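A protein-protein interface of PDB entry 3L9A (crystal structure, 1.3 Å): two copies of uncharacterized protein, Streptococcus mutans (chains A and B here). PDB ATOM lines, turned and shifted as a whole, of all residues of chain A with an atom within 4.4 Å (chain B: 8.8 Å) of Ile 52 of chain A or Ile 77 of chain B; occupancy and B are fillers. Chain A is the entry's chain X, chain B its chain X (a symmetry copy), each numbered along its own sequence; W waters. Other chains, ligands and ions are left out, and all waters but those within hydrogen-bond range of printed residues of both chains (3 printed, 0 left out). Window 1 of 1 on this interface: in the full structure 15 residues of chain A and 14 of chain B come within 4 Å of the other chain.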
ATOM      1  N   PHE A  12      19.470  22.768  18.721  1.00  0.00           N
ATOM      2  CA  PHE A  12      18.426  21.750  18.720  1.00  0.00           C
ATOM      3  C   PHE A  12      17.040  22.382  18.802  1.00  0.00           C
ATOM      4  O   PHE A  12      16.846  23.418  19.459  1.00  0.00           O
ATOM      5  CB  PHE A  12      18.532  20.864  19.965  1.00  0.00           C
ATOM      6  CG  PHE A  12      19.665  19.868  19.970  1.00  0.00           C
ATOM      7  CD1 PHE A  12      19.817  18.923  18.952  1.00  0.00           C
ATOM      8  CD2 PHE A  12      20.527  19.818  21.060  1.00  0.00           C
ATOM      9  CE1 PHE A  12      20.841  17.965  19.020  1.00  0.00           C
ATOM     10  CE2 PHE A  12      21.542  18.867  21.130  1.00  0.00           C
ATOM     11  CZ  PHE A  12      21.696  17.943  20.113  1.00  0.00           C
ATOM     12  N   HIS A  33      18.556  18.174  15.093  1.00  0.00           N
ATOM     13  CA  HIS A  33      19.799  18.928  15.076  1.00  0.00           C
ATOM     14  C   HIS A  33      19.770  19.842  13.864  1.00  0.00           C
ATOM     15  O   HIS A  33      19.625  19.369  12.732  1.00  0.00           O
ATOM     16  CB  HIS A  33      20.998  17.994  14.973  1.00  0.00           C
ATOM     17  CG  HIS A  33      22.310  18.710  15.018  1.00  0.00           C
ATOM     18  ND1 HIS A  33      23.058  18.974  13.888  1.00  0.00           N
ATOM     19  CD2 HIS A  33      22.989  19.257  16.057  1.00  0.00           C
ATOM     20  CE1 HIS A  33      24.158  19.626  14.240  1.00  0.00           C
ATOM     21  NE2 HIS A  33      24.147  19.798  15.551  1.00  0.00           N
ATOM     22  N   GLN A  38      25.657  24.235   7.546  1.00  0.00           N
ATOM     23  CA  GLN A  38      25.548  23.146   6.575  1.00  0.00           C
ATOM     24  C   GLN A  38      24.196  23.108   5.858  1.00  0.00           C
ATOM     25  O   GLN A  38      23.949  22.211   5.051  1.00  0.00           O
ATOM     26  CB  GLN A  38      25.818  21.813   7.268  1.00  0.00           C
ATOM     27  CG  GLN A  38      27.218  21.729   7.878  1.00  0.00           C
ATOM     28  CD  GLN A  38      27.638  20.303   8.193  1.00  0.00           C
ATOM     29  OE1 GLN A  38      26.801  19.400   8.293  1.00  0.00           O
ATOM     30  NE2 GLN A  38      28.935  20.087   8.337  1.00  0.00           N
ATOM     31  N   ARG A  40      21.415  22.108   6.904  1.00  0.00           N
ATOM     32  CA  ARG A  40      20.898  20.758   7.129  1.00  0.00           C
ATOM     33  C   ARG A  40      20.335  20.615   8.533  1.00  0.00           C
ATOM     34  O   ARG A  40      20.987  21.011   9.509  1.00  0.00           O
ATOM     35  CB  ARG A  40      22.008  19.713   6.926  1.00  0.00           C
ATOM     36  CG  ARG A  40      21.561  18.264   7.216  1.00  0.00           C
ATOM     37  CD  ARG A  40      22.680  17.262   6.988  1.00  0.00           C
ATOM     38  NE  ARG A  40      22.305  15.896   7.371  1.00  0.00           N
ATOM     39  CZ  ARG A  40      22.975  15.123   8.226  1.00  0.00           C
ATOM     40  NH1 ARG A  40      24.068  15.560   8.838  1.00  0.00           N
ATOM     41  NH2 ARG A  40      22.532  13.894   8.482  1.00  0.00           N
ATOM     42  N   PHE A  42      18.343  17.405  10.858  1.00  0.00           N
ATOM     43  CA  PHE A  42      17.912  16.014  10.811  1.00  0.00           C
ATOM     44  C   PHE A  42      17.511  15.511  12.184  1.00  0.00           C
ATOM     45  O   PHE A  42      17.875  16.084  13.207  1.00  0.00           O
ATOM     46  CB  PHE A  42      18.957  15.104  10.123  1.00  0.00           C
ATOM     47  CG  PHE A  42      20.143  14.726  10.970  1.00  0.00           C
ATOM     48  CD1 PHE A  42      20.286  13.417  11.422  1.00  0.00           C
ATOM     49  CD2 PHE A  42      21.158  15.642  11.239  1.00  0.00           C
ATOM     50  CE1 PHE A  42      21.398  13.037  12.166  1.00  0.00           C
ATOM     51  CE2 PHE A  42      22.273  15.272  11.997  1.00  0.00           C
ATOM     52  CZ  PHE A  42      22.399  13.965  12.454  1.00  0.00           C
ATOM     53  N   VAL A  44      17.825  13.264  15.125  1.00  0.00           N
ATOM     54  CA  VAL A  44      18.881  12.487  15.766  1.00  0.00           C
ATOM     55  C   VAL A  44      18.305  11.425  16.684  1.00  0.00           C
ATOM     56  O   VAL A  44      17.294  11.647  17.336  1.00  0.00           O
ATOM     57  CB  VAL A  44      19.882  13.384  16.567  1.00  0.00           C
ATOM     58  CG1 VAL A  44      20.685  14.258  15.618  1.00  0.00           C
ATOM     59  CG2 VAL A  44      19.189  14.217  17.659  1.00  0.00           C
ATOM     60  N   GLN A  48      23.129   9.900  19.191  1.00  0.00           N
ATOM     61  CA  GLN A  48      23.646  11.019  18.405  1.00  0.00           C
ATOM     62  C   GLN A  48      23.461  12.360  19.123  1.00  0.00           C
ATOM     63  O   GLN A  48      24.365  13.192  19.136  1.00  0.00           O
ATOM     64  CB  GLN A  48      22.979  11.065  17.040  1.00  0.00           C
ATOM     65  CG  GLN A  48      23.382   9.933  16.105  1.00  0.00           C
ATOM     66  CD  GLN A  48      22.605   9.992  14.802  1.00  0.00           C
ATOM     67  OE1 GLN A  48      21.402  10.250  14.804  1.00  0.00           O
ATOM     68  NE2 GLN A  48      23.291   9.772  13.688  1.00  0.00           N
ATOM     69  N   GLU A  49      22.282  12.567  19.714  1.00  0.00           N
ATOM     70  CA  GLU A  49      22.023  13.748  20.520  1.00  0.00           C
ATOM     71  C   GLU A  49      23.103  13.897  21.598  1.00  0.00           C
ATOM     72  O   GLU A  49      23.663  14.982  21.803  1.00  0.00           O
ATOM     73  CB  GLU A  49      20.640  13.607  21.162  1.00  0.00           C
ATOM     74  CG  GLU A  49      20.235  14.791  22.007  1.00  0.00           C
ATOM     75  CD  GLU A  49      18.867  14.608  22.650  1.00  0.00           C
ATOM     76  OE1 GLU A  49      18.257  13.531  22.491  1.00  0.00           O
ATOM     77  OE2 GLU A  49      18.399  15.533  23.338  1.00  0.00           O
ATOM     78  N   ASN A  50      23.407  12.793  22.274  1.00  0.00           N
ATOM     79  CA  ASN A  50      24.409  12.820  23.337  1.00  0.00           C
ATOM     80  C   ASN A  50      25.814  13.066  22.819  1.00  0.00           C
ATOM     81  O   ASN A  50      26.576  13.822  23.421  1.00  0.00           O
ATOM     82  CB  ASN A  50      24.314  11.562  24.181  1.00  0.00           C
ATOM     83  CG  ASN A  50      23.029  11.516  24.950  1.00  0.00           C
ATOM     84  OD1 ASN A  50      22.473  12.562  25.293  1.00  0.00           O
ATOM     85  ND2 ASN A  50      22.539  10.315  25.217  1.00  0.00           N
ATOM     86  N   PHE A  51      26.144  12.449  21.691  1.00  0.00           N
ATOM     87  CA  PHE A  51      27.421  12.690  21.032  1.00  0.00           C
ATOM     88  C   PHE A  51      27.610  14.174  20.723  1.00  0.00           C
ATOM     89  O   PHE A  51      28.663  14.748  21.008  1.00  0.00           O
ATOM     90  CB  PHE A  51      27.495  11.868  19.745  1.00  0.00           C
ATOM     91  CG  PHE A  51      28.762  12.080  18.973  1.00  0.00           C
ATOM     92  CD1 PHE A  51      29.849  11.241  19.166  1.00  0.00           C
ATOM     93  CD2 PHE A  51      28.886  13.138  18.073  1.00  0.00           C
ATOM     94  CE1 PHE A  51      31.032  11.442  18.454  1.00  0.00           C
ATOM     95  CE2 PHE A  51      30.074  13.347  17.373  1.00  0.00           C
ATOM     96  CZ  PHE A  51      31.141  12.493  17.568  1.00  0.00           C
ATOM     97  N   ILE A  52      26.582  14.793  20.147  1.00  0.00           N
ATOM     98  CA  ILE A  52      26.638  16.204  19.803  1.00  0.00           C
ATOM     99  C   ILE A  52      26.983  17.028  21.041  1.00  0.00           C
ATOM    100  O   ILE A  52      27.789  17.949  20.953  1.00  0.00           O
ATOM    101  CB  ILE A  52      25.322  16.662  19.162  1.00  0.00           C
ATOM    102  CG1 ILE A  52      25.201  16.065  17.756  1.00  0.00           C
ATOM    103  CG2 ILE A  52      25.237  18.192  19.103  1.00  0.00           C
ATOM    104  CD1 ILE A  52      23.769  15.984  17.245  1.00  0.00           C
ATOM    105  N   LYS A  53      26.404  16.674  22.190  1.00  0.00           N
ATOM    106  CA  LYS A  53      26.664  17.430  23.408  1.00  0.00           C
ATOM    107  C   LYS A  53      28.061  17.190  23.976  1.00  0.00           C
ATOM    108  O   LYS A  53      28.527  17.985  24.784  1.00  0.00           O
ATOM    109  CB  LYS A  53      25.559  17.198  24.433  1.00  0.00           C
ATOM    110  CG  LYS A  53      24.252  17.824  23.962  1.00  0.00           C
ATOM    111  CD  LYS A  53      23.143  17.798  24.992  1.00  0.00           C
ATOM    112  CE  LYS A  53      22.627  16.409  25.269  1.00  0.00           C
ATOM    113  NZ  LYS A  53      21.422  16.522  26.159  1.00  0.00           N
ATOM    114  N   GLN A  54      28.738  16.116  23.564  1.00  0.00           N
ATOM    115  CA  GLN A  54      30.159  15.966  23.896  1.00  0.00           C
ATOM    116  C   GLN A  54      31.040  16.901  23.065  1.00  0.00           C
ATOM    117  O   GLN A  54      31.955  17.545  23.592  1.00  0.00           O
ATOM    118  CB  GLN A  54      30.632  14.528  23.687  1.00  0.00           C
ATOM    119  CG  GLN A  54      32.058  14.294  24.200  1.00  0.00           C
ATOM    120  CD  GLN A  54      32.502  12.859  24.056  1.00  0.00           C
ATOM    121  OE1 GLN A  54      31.695  11.939  24.139  1.00  0.00           O
ATOM    122  NE2 GLN A  54      33.796  12.658  23.863  1.00  0.00           N
ATOM    123  N   VAL A  55      30.784  16.964  21.762  1.00  0.00           N
ATOM    124  CA  VAL A  55      31.667  17.741  20.904  1.00  0.00           C
ATOM    125  C   VAL A  55      31.278  19.220  20.862  1.00  0.00           C
ATOM    126  O   VAL A  55      32.130  20.056  20.556  1.00  0.00           O
ATOM    127  CB  VAL A  55      31.850  17.101  19.499  1.00  0.00           C
ATOM    128  CG1 VAL A  55      32.298  15.642  19.618  1.00  0.00           C
ATOM    129  CG2 VAL A  55      30.584  17.191  18.693  1.00  0.00           C
ATOM    130  N   ASN A  56      30.021  19.529  21.203  1.00  0.00           N
ATOM    131  CA  ASN A  56      29.497  20.883  21.165  1.00  0.00           C
ATOM    132  C   ASN A  56      28.728  21.124  22.450  1.00  0.00           C
ATOM    133  O   ASN A  56      27.495  21.198  22.464  1.00  0.00           O
ATOM    134  CB  ASN A  56      28.558  20.989  19.960  1.00  0.00           C
ATOM    135  CG  ASN A  56      28.051  22.400  19.716  1.00  0.00           C
ATOM    136  OD1 ASN A  56      28.378  23.347  20.442  1.00  0.00           O
ATOM    137  ND2 ASN A  56      27.244  22.550  18.680  1.00  0.00           N
ATOM    138  N   ILE A  59      25.720  23.702  22.964  1.00  0.00           N
ATOM    139  CA  ILE A  59      24.552  23.718  22.084  1.00  0.00           C
ATOM    140  C   ILE A  59      23.278  23.924  22.911  1.00  0.00           C
ATOM    141  O   ILE A  59      23.142  23.386  24.018  1.00  0.00           O
ATOM    142  CB  ILE A  59      24.483  22.441  21.213  1.00  0.00           C
ATOM    143  CG1 ILE A  59      23.451  22.639  20.093  1.00  0.00           C
ATOM    144  CG2 ILE A  59      24.216  21.177  22.056  1.00  0.00           C
ATOM    145  CD1 ILE A  59      23.456  21.547  19.031  1.00  0.00           C
ATOM    146  N   MET B   8      29.013  23.923  13.744  1.00  0.00           N
ATOM    147  CA  MET B   8      29.913  23.583  14.880  1.00  0.00           C
ATOM    148  C   MET B   8      31.327  24.109  14.642  1.00  0.00           C
ATOM    149  O   MET B   8      31.859  23.976  13.538  1.00  0.00           O
ATOM    150  CB  MET B   8      29.926  22.066  15.106  1.00  0.00           C
ATOM    151  CG  MET B   8      30.993  21.555  16.075  1.00  0.00           C
ATOM    152  SD  MET B   8      30.831  22.316  17.869  1.00  0.00           S
ATOM    153  CE  MET B   8      32.610  21.881  18.494  1.00  0.00           C
ATOM    154  N   PHE B  11      37.275  21.290  16.120  1.00  0.00           N
ATOM    155  CA  PHE B  11      37.697  20.601  17.340  1.00  0.00           C
ATOM    156  C   PHE B  11      38.742  19.558  17.010  1.00  0.00           C
ATOM    157  O   PHE B  11      38.891  19.162  15.850  1.00  0.00           O
ATOM    158  CB  PHE B  11      36.507  19.983  18.096  1.00  0.00           C
ATOM    159  CG  PHE B  11      35.690  18.981  17.297  1.00  0.00           C
ATOM    160  CD1 PHE B  11      35.987  17.624  17.338  1.00  0.00           C
ATOM    161  CD2 PHE B  11      34.585  19.388  16.564  1.00  0.00           C
ATOM    162  CE1 PHE B  11      35.201  16.691  16.654  1.00  0.00           C
ATOM    163  CE2 PHE B  11      33.805  18.456  15.857  1.00  0.00           C
ATOM    164  CZ  PHE B  11      34.113  17.113  15.917  1.00  0.00           C
ATOM    165  N   PRO B  36      33.780  20.862  10.994  1.00  0.00           N
ATOM    166  CA  PRO B  36      32.443  20.685  10.421  1.00  0.00           C
ATOM    167  C   PRO B  36      32.099  21.706   9.336  1.00  0.00           C
ATOM    168  O   PRO B  36      31.476  21.345   8.335  1.00  0.00           O
ATOM    169  CB  PRO B  36      31.528  20.815  11.646  1.00  0.00           C
ATOM    170  CG  PRO B  36      32.403  20.285  12.770  1.00  0.00           C
ATOM    171  CD  PRO B  36      33.743  20.912  12.465  1.00  0.00           C
ATOM    172  N   LYS B  39      33.577  20.581   6.291  1.00  0.00           N
ATOM    173  CA  LYS B  39      33.351  19.138   6.082  1.00  0.00           C
ATOM    174  C   LYS B  39      34.668  18.379   5.847  1.00  0.00           C
ATOM    175  O   LYS B  39      34.767  17.527   4.964  1.00  0.00           O
ATOM    176  CB  LYS B  39      32.342  18.902   4.948  1.00  0.00           C
ATOM    177  CG  LYS B  39      30.943  19.385   5.305  1.00  0.00           C
ATOM    178  CD  LYS B  39      29.958  19.159   4.160  1.00  0.00           C
ATOM    179  CE  LYS B  39      28.547  19.593   4.546  1.00  0.00           C
ATOM    180  NZ  LYS B  39      27.636  19.570   3.361  1.00  0.00           N
ATOM    181  N   VAL B  62      38.032  17.183  22.235  1.00  0.00           N
ATOM    182  CA  VAL B  62      36.748  16.743  22.792  1.00  0.00           C
ATOM    183  C   VAL B  62      36.725  15.246  23.082  1.00  0.00           C
ATOM    184  O   VAL B  62      35.861  14.779  23.824  1.00  0.00           O
ATOM    185  CB  VAL B  62      35.563  17.115  21.882  1.00  0.00           C
ATOM    186  CG1 VAL B  62      35.458  18.627  21.734  1.00  0.00           C
ATOM    187  CG2 VAL B  62      35.683  16.446  20.526  1.00  0.00           C
ATOM    188  N   ALA B  69      34.161   4.048  15.801  1.00  0.00           N
ATOM    189  CA  ALA B  69      32.739   4.350  16.011  1.00  0.00           C
ATOM    190  C   ALA B  69      32.519   5.828  16.311  1.00  0.00           C
ATOM    191  O   ALA B  69      31.516   6.413  15.893  1.00  0.00           O
ATOM    192  CB  ALA B  69      32.153   3.483  17.121  1.00  0.00           C
ATOM    193  N   PHE B  70      33.457   6.441  17.029  1.00  0.00           N
ATOM    194  CA  PHE B  70      33.382   7.869  17.310  1.00  0.00           C
ATOM    195  C   PHE B  70      33.534   8.684  16.019  1.00  0.00           C
ATOM    196  O   PHE B  70      32.777   9.635  15.768  1.00  0.00           O
ATOM    197  CB  PHE B  70      34.456   8.245  18.338  1.00  0.00           C
ATOM    198  CG  PHE B  70      34.208   9.573  19.007  1.00  0.00           C
ATOM    199  CD1 PHE B  70      34.683  10.756  18.457  1.00  0.00           C
ATOM    200  CD2 PHE B  70      33.474   9.629  20.190  1.00  0.00           C
ATOM    201  CE1 PHE B  70      34.432  11.987  19.085  1.00  0.00           C
ATOM    202  CE2 PHE B  70      33.220  10.846  20.828  1.00  0.00           C
ATOM    203  CZ  PHE B  70      33.692  12.021  20.273  1.00  0.00           C
ATOM    204  N   LEU B  71      34.497   8.302  15.183  1.00  0.00           N
ATOM    205  CA  LEU B  71      34.660   8.989  13.905  1.00  0.00           C
ATOM    206  C   LEU B  71      33.427   8.824  13.013  1.00  0.00           C
ATOM    207  O   LEU B  71      33.046   9.752  12.315  1.00  0.00           O
ATOM    208  CB  LEU B  71      35.935   8.547  13.183  1.00  0.00           C
ATOM    209  CG  LEU B  71      37.255   8.660  13.958  1.00  0.00           C
ATOM    210  CD1 LEU B  71      38.438   8.435  13.024  1.00  0.00           C
ATOM    211  CD2 LEU B  71      37.400   9.995  14.673  1.00  0.00           C
ATOM    212  N   GLN B  72      32.783   7.661  13.075  1.00  0.00           N
ATOM    213  CA  GLN B  72      31.569   7.440  12.299  1.00  0.00           C
ATOM    214  C   GLN B  72      30.440   8.377  12.728  1.00  0.00           C
ATOM    215  O   GLN B  72      29.680   8.847  11.889  1.00  0.00           O
ATOM    216  CB  GLN B  72      31.140   5.969  12.367  1.00  0.00           C
ATOM    217  CG  GLN B  72      29.900   5.646  11.509  1.00  0.00           C
ATOM    218  CD  GLN B  72      30.115   5.915  10.028  1.00  0.00           C
ATOM    219  OE1 GLN B  72      31.247   5.890   9.542  1.00  0.00           O
ATOM    220  NE2 GLN B  72      29.029   6.167   9.297  1.00  0.00           N
ATOM    221  N   ARG B  73      30.354   8.686  14.022  1.00  0.00           N
ATOM    222  CA  ARG B  73      29.398   9.695  14.468  1.00  0.00           C
ATOM    223  C   ARG B  73      29.703  11.058  13.852  1.00  0.00           C
ATOM    224  O   ARG B  73      28.791  11.793  13.500  1.00  0.00           O
ATOM    225  CB  ARG B  73      29.381   9.787  15.989  1.00  0.00           C
ATOM    226  CG  ARG B  73      28.755   8.615  16.703  1.00  0.00           C
ATOM    227  CD  ARG B  73      27.225   8.650  16.623  1.00  0.00           C
ATOM    228  NE  ARG B  73      26.671   7.566  17.431  1.00  0.00           N
ATOM    229  CZ  ARG B  73      25.782   6.666  17.018  1.00  0.00           C
ATOM    230  NH1 ARG B  73      25.273   6.705  15.792  1.00  0.00           N
ATOM    231  NH2 ARG B  73      25.379   5.728  17.866  1.00  0.00           N
ATOM    232  N   ILE B  74      30.981  11.404  13.735  1.00  0.00           N
ATOM    233  CA  ILE B  74      31.359  12.658  13.104  1.00  0.00           C
ATOM    234  C   ILE B  74      30.872  12.677  11.641  1.00  0.00           C
ATOM    235  O   ILE B  74      30.352  13.690  11.164  1.00  0.00           O
ATOM    236  CB  ILE B  74      32.874  12.920  13.210  1.00  0.00           C
ATOM    237  CG1 ILE B  74      33.289  13.056  14.681  1.00  0.00           C
ATOM    238  CG2 ILE B  74      33.242  14.170  12.411  1.00  0.00           C
ATOM    239  CD1 ILE B  74      34.780  13.149  14.906  1.00  0.00           C
ATOM    240  N   VAL B  75      31.037  11.559  10.932  1.00  0.00           N
ATOM    241  CA  VAL B  75      30.523  11.438   9.571  1.00  0.00           C
ATOM    242  C   VAL B  75      28.996  11.628   9.541  1.00  0.00           C
ATOM    243  O   VAL B  75      28.472  12.400   8.726  1.00  0.00           O
ATOM    244  CB  VAL B  75      30.937  10.091   8.939  1.00  0.00           C
ATOM    245  CG1 VAL B  75      30.234   9.865   7.605  1.00  0.00           C
ATOM    246  CG2 VAL B  75      32.449  10.029   8.774  1.00  0.00           C
ATOM    247  N   GLU B  76      28.290  10.955  10.445  1.00  0.00           N
ATOM    248  CA  GLU B  76      26.824  11.016  10.458  1.00  0.00           C
ATOM    249  C   GLU B  76      26.298  12.421  10.703  1.00  0.00           C
ATOM    250  O   GLU B  76      25.377  12.887  10.020  1.00  0.00           O
ATOM    251  CB  GLU B  76      26.259  10.118  11.563  1.00  0.00           C
ATOM    252  CG  GLU B  76      26.415   8.640  11.312  1.00  0.00           C
ATOM    253  CD  GLU B  76      26.233   7.807  12.566  1.00  0.00           C
ATOM    254  OE1 GLU B  76      25.860   8.353  13.625  1.00  0.00           O
ATOM    255  OE2 GLU B  76      26.482   6.592  12.479  1.00  0.00           O
ATOM    256  N   ILE B  77      26.874  13.075  11.709  1.00  0.00           N
ATOM    257  CA  ILE B  77      26.325  14.327  12.191  1.00  0.00           C
ATOM    258  C   ILE B  77      26.834  15.496  11.368  1.00  0.00           C
ATOM    259  O   ILE B  77      26.064  16.402  11.055  1.00  0.00           O
ATOM    260  CB  ILE B  77      26.600  14.562  13.711  1.00  0.00           C
ATOM    261  CG1 ILE B  77      25.678  13.711  14.593  1.00  0.00           C
ATOM    262  CG2 ILE B  77      26.292  15.997  14.093  1.00  0.00           C
ATOM    263  CD1 ILE B  77      25.734  12.265  14.361  1.00  0.00           C
ATOM    264  N   TYR B  78      28.115  15.480  11.009  1.00  0.00           N
ATOM    265  CA  TYR B  78      28.769  16.621  10.377  1.00  0.00           C
ATOM    266  C   TYR B  78      29.169  16.415   8.925  1.00  0.00           C
ATOM    267  O   TYR B  78      29.696  17.342   8.313  1.00  0.00           O
ATOM    268  CB  TYR B  78      29.956  17.120  11.233  1.00  0.00           C
ATOM    269  CG  TYR B  78      29.535  17.508  12.634  1.00  0.00           C
ATOM    270  CD1 TYR B  78      28.714  18.623  12.847  1.00  0.00           C
ATOM    271  CD2 TYR B  78      29.942  16.771  13.744  1.00  0.00           C
ATOM    272  CE1 TYR B  78      28.297  18.983  14.125  1.00  0.00           C
ATOM    273  CE2 TYR B  78      29.535  17.128  15.030  1.00  0.00           C
ATOM    274  CZ  TYR B  78      28.710  18.234  15.207  1.00  0.00           C
ATOM    275  OH  TYR B  78      28.313  18.570  16.480  1.00  0.00           O
ATOM    276  N   GLN B  79      28.980  15.209   8.395  1.00  0.00           N
ATOM    277  CA  GLN B  79      29.189  14.977   6.962  1.00  0.00           C
ATOM    278  C   GLN B  79      30.653  15.221   6.567  1.00  0.00           C
ATOM    279  O   GLN B  79      30.955  15.603   5.441  1.00  0.00           O
ATOM    280  CB  GLN B  79      28.230  15.862   6.147  1.00  0.00           C
ATOM    281  CG  GLN B  79      26.776  15.745   6.618  1.00  0.00           C
ATOM    282  CD  GLN B  79      25.824  16.492   5.723  1.00  0.00           C
ATOM    283  OE1 GLN B  79      25.203  15.898   4.848  1.00  0.00           O
ATOM    284  NE2 GLN B  79      25.714  17.806   5.925  1.00  0.00           N
ATOM    285  N   VAL B  80      31.557  14.961   7.508  1.00  0.00           N
ATOM    286  CA  VAL B  80      32.974  15.261   7.341  1.00  0.00           C
ATOM    287  C   VAL B  80      33.663  14.213   6.473  1.00  0.00           C
ATOM    288  O   VAL B  80      33.451  13.011   6.669  1.00  0.00           O
ATOM    289  CB  VAL B  80      33.641  15.369   8.731  1.00  0.00           C
ATOM    290  CG1 VAL B  80      35.145  15.305   8.641  1.00  0.00           C
ATOM    291  CG2 VAL B  80      33.204  16.644   9.417  1.00  0.00           C
HETATM  292  O   HOH W   1      24.876  19.830   4.206  1.00  0.00           O
HETATM  293  O   HOH W   2      25.407  19.132  10.999  1.00  0.00           O
HETATM  294  O   HOH W   3      26.599  20.640  16.592  1.00  0.00           O
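O of Phe 42 of chain A is in hydrogen-bond range of N of His 33 of chain A, at 2.9 Å. The guanidinium group of Arg 73 of chain B lies within salt-bridge range of the side-chain carboxylate of Glu 76 of chain B (2.8 Å). The backbone NH (N) of Gln 79 of chain B sits at hydrogen-bond distance from the backbone carbonyl oxygen (O) of Ile 74 of chain B, at 3.4 Å.
Among the printed residues, merely in contact across the chains: Gln 38 of chain A with Lys 39 of chain B (3.7 Å), Arg 40 of chain A with Gln 79 of chain B (3.3 Å), Phe 42 of chain A with Glu 76 of chain B (3.99 Å), Phe 42 of chain A with Ile 77 of chain B (3.9 Å), Gln 48 of chain A with Arg 73 of chain B (3.8 Å), Gln 48 of chain A with Ile 77 of chain B (3.6 Å), Phe 51 of chain A with Phe 70 of chain B (3.3 Å), Phe 51 of chain A with Arg 73 of chain B (3.4 Å), Phe 51 of chain A with Ile 74 of chain B (3.6 Å), Ile 52 of chain A with Ile 77 of chain B (3.8 Å), Gln 54 of chain A with Phe 70 of chain B (3.6 Å), Val 55 of chain A with Val 62 of chain B (3.6 Å), Val 55 of chain A with Phe 70 of chain B (3.9 Å) and Val 55 of chain A with Tyr 78 of chain B (3.5 Å).
Water W3 lies within hydrogen-bond range of OH of Tyr 78 of chain B (2.7 Å), NE2 of His 33 of chain A (2.8 Å) and ND2 of Asn 56 of chain A (2.9 Å). Water W1 lies within hydrogen-bond range of the backbone carbonyl oxygen of Gln 38 of chain A, the side-chain amide nitrogen of Gln 79 of chain B and the side-chain amino group of Lys 39 of chain B. Water W2 lies within hydrogen-bond range of O of Ile 77 of chain B and OE1 of Gln 38 of chain A.
The backbone carbonyl oxygen (O) of Pro 36 of chain B is in hydrogen-bond range of the side-chain amide nitrogen (NE2) of Gln 38 of chain A, at 2.8 Å. The backbone carbonyl oxygen (O) of Tyr 78 of chain B sits at hydrogen-bond distance from the side-chain amide nitrogen (NE2) of Gln 38 of chain A, 2.8 Å away. The side-chain amide oxygen (OE1) of Gln 38 of chain A sits at hydrogen-bond distance from the side-chain amide nitrogen (NE2) of Gln 79 of chain B. The guanidinium group of Arg 40 of chain A lies within hydrogen-bond range of the backbone carbonyl oxygen of Glu 76 of chain B (3.2 Å). NH1 of Arg 40 of chain A lies within hydrogen-bond range of O of Ile 77 of chain B (3.1 Å). The side-chain amide nitrogen of Gln 48 of chain A lies within hydrogen-bond range of the side-chain carboxylate of Glu 76 of chain B (2.9 Å). The side-chain amide nitrogen (NE2) of Gln 54 of chain A sits at hydrogen-bond distance from the backbone carbonyl oxygen (O) of Val 62 of chain B (3.0 Å). SD of Met 8 of chain B sits close to ND2 of Asn 56 of chain A, at 3.7 Å. The backbone carbonyl oxygen of Val 55 of chain A sits close to the side-chain sulfur of Met 8 of chain B, 3.7 Å away.
Of the printed residues of chain B, Arg 40 of chain A touches Glu 76, Ile 77 and Gln 79. Of the printed residues of chain B, Ile 52 of chain A touches Ile 77. Of the printed residues of chain A, Met 8 of chain B touches Val 55 and Asn 56. Of the printed residues of chain A, Val 62 of chain B touches Gln 54 and Val 55. Printed residues of chain A within 4 Å of Ile 77 of chain B: Arg 40 (3.1 Å), Phe 42 (3.9 Å), Gln 48 (3.6 Å) and Ile 52 (3.8 Å). The nearest printed residue of chain B that does not touch Ile 52 of chain A is Tyr 78 of chain B (4.1 Å). The nearest printed residue of chain A that does not touch Ile 77 of chain B is Gln 38 of chain A (4.1 Å).
Hydrophobic or aromatic side chains of chain A within 4 Å of the printed part of chain B: Phe 42, Phe 51, Ile 52 and Val 55. Of the 17 printed residues of chain B, 11 touch a printed residue of chain A. Hydrophobic or aromatic side chains of chain B that line the printed part of chain A: Met 8, Val 62, Phe 70, Ile 74, Ile 77 and Tyr 78. Among the printed residues, 23 pairs touch across the chains. Among the printed residues, no Asp or Glu carboxylate lies within 4 Å of a Lys or Arg side-chain nitrogen of the other chain.
No position is printed for both chains. Of the 23 pairs that touch across the chains among the printed residues, none has its exchanged pair printed and touching as well.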
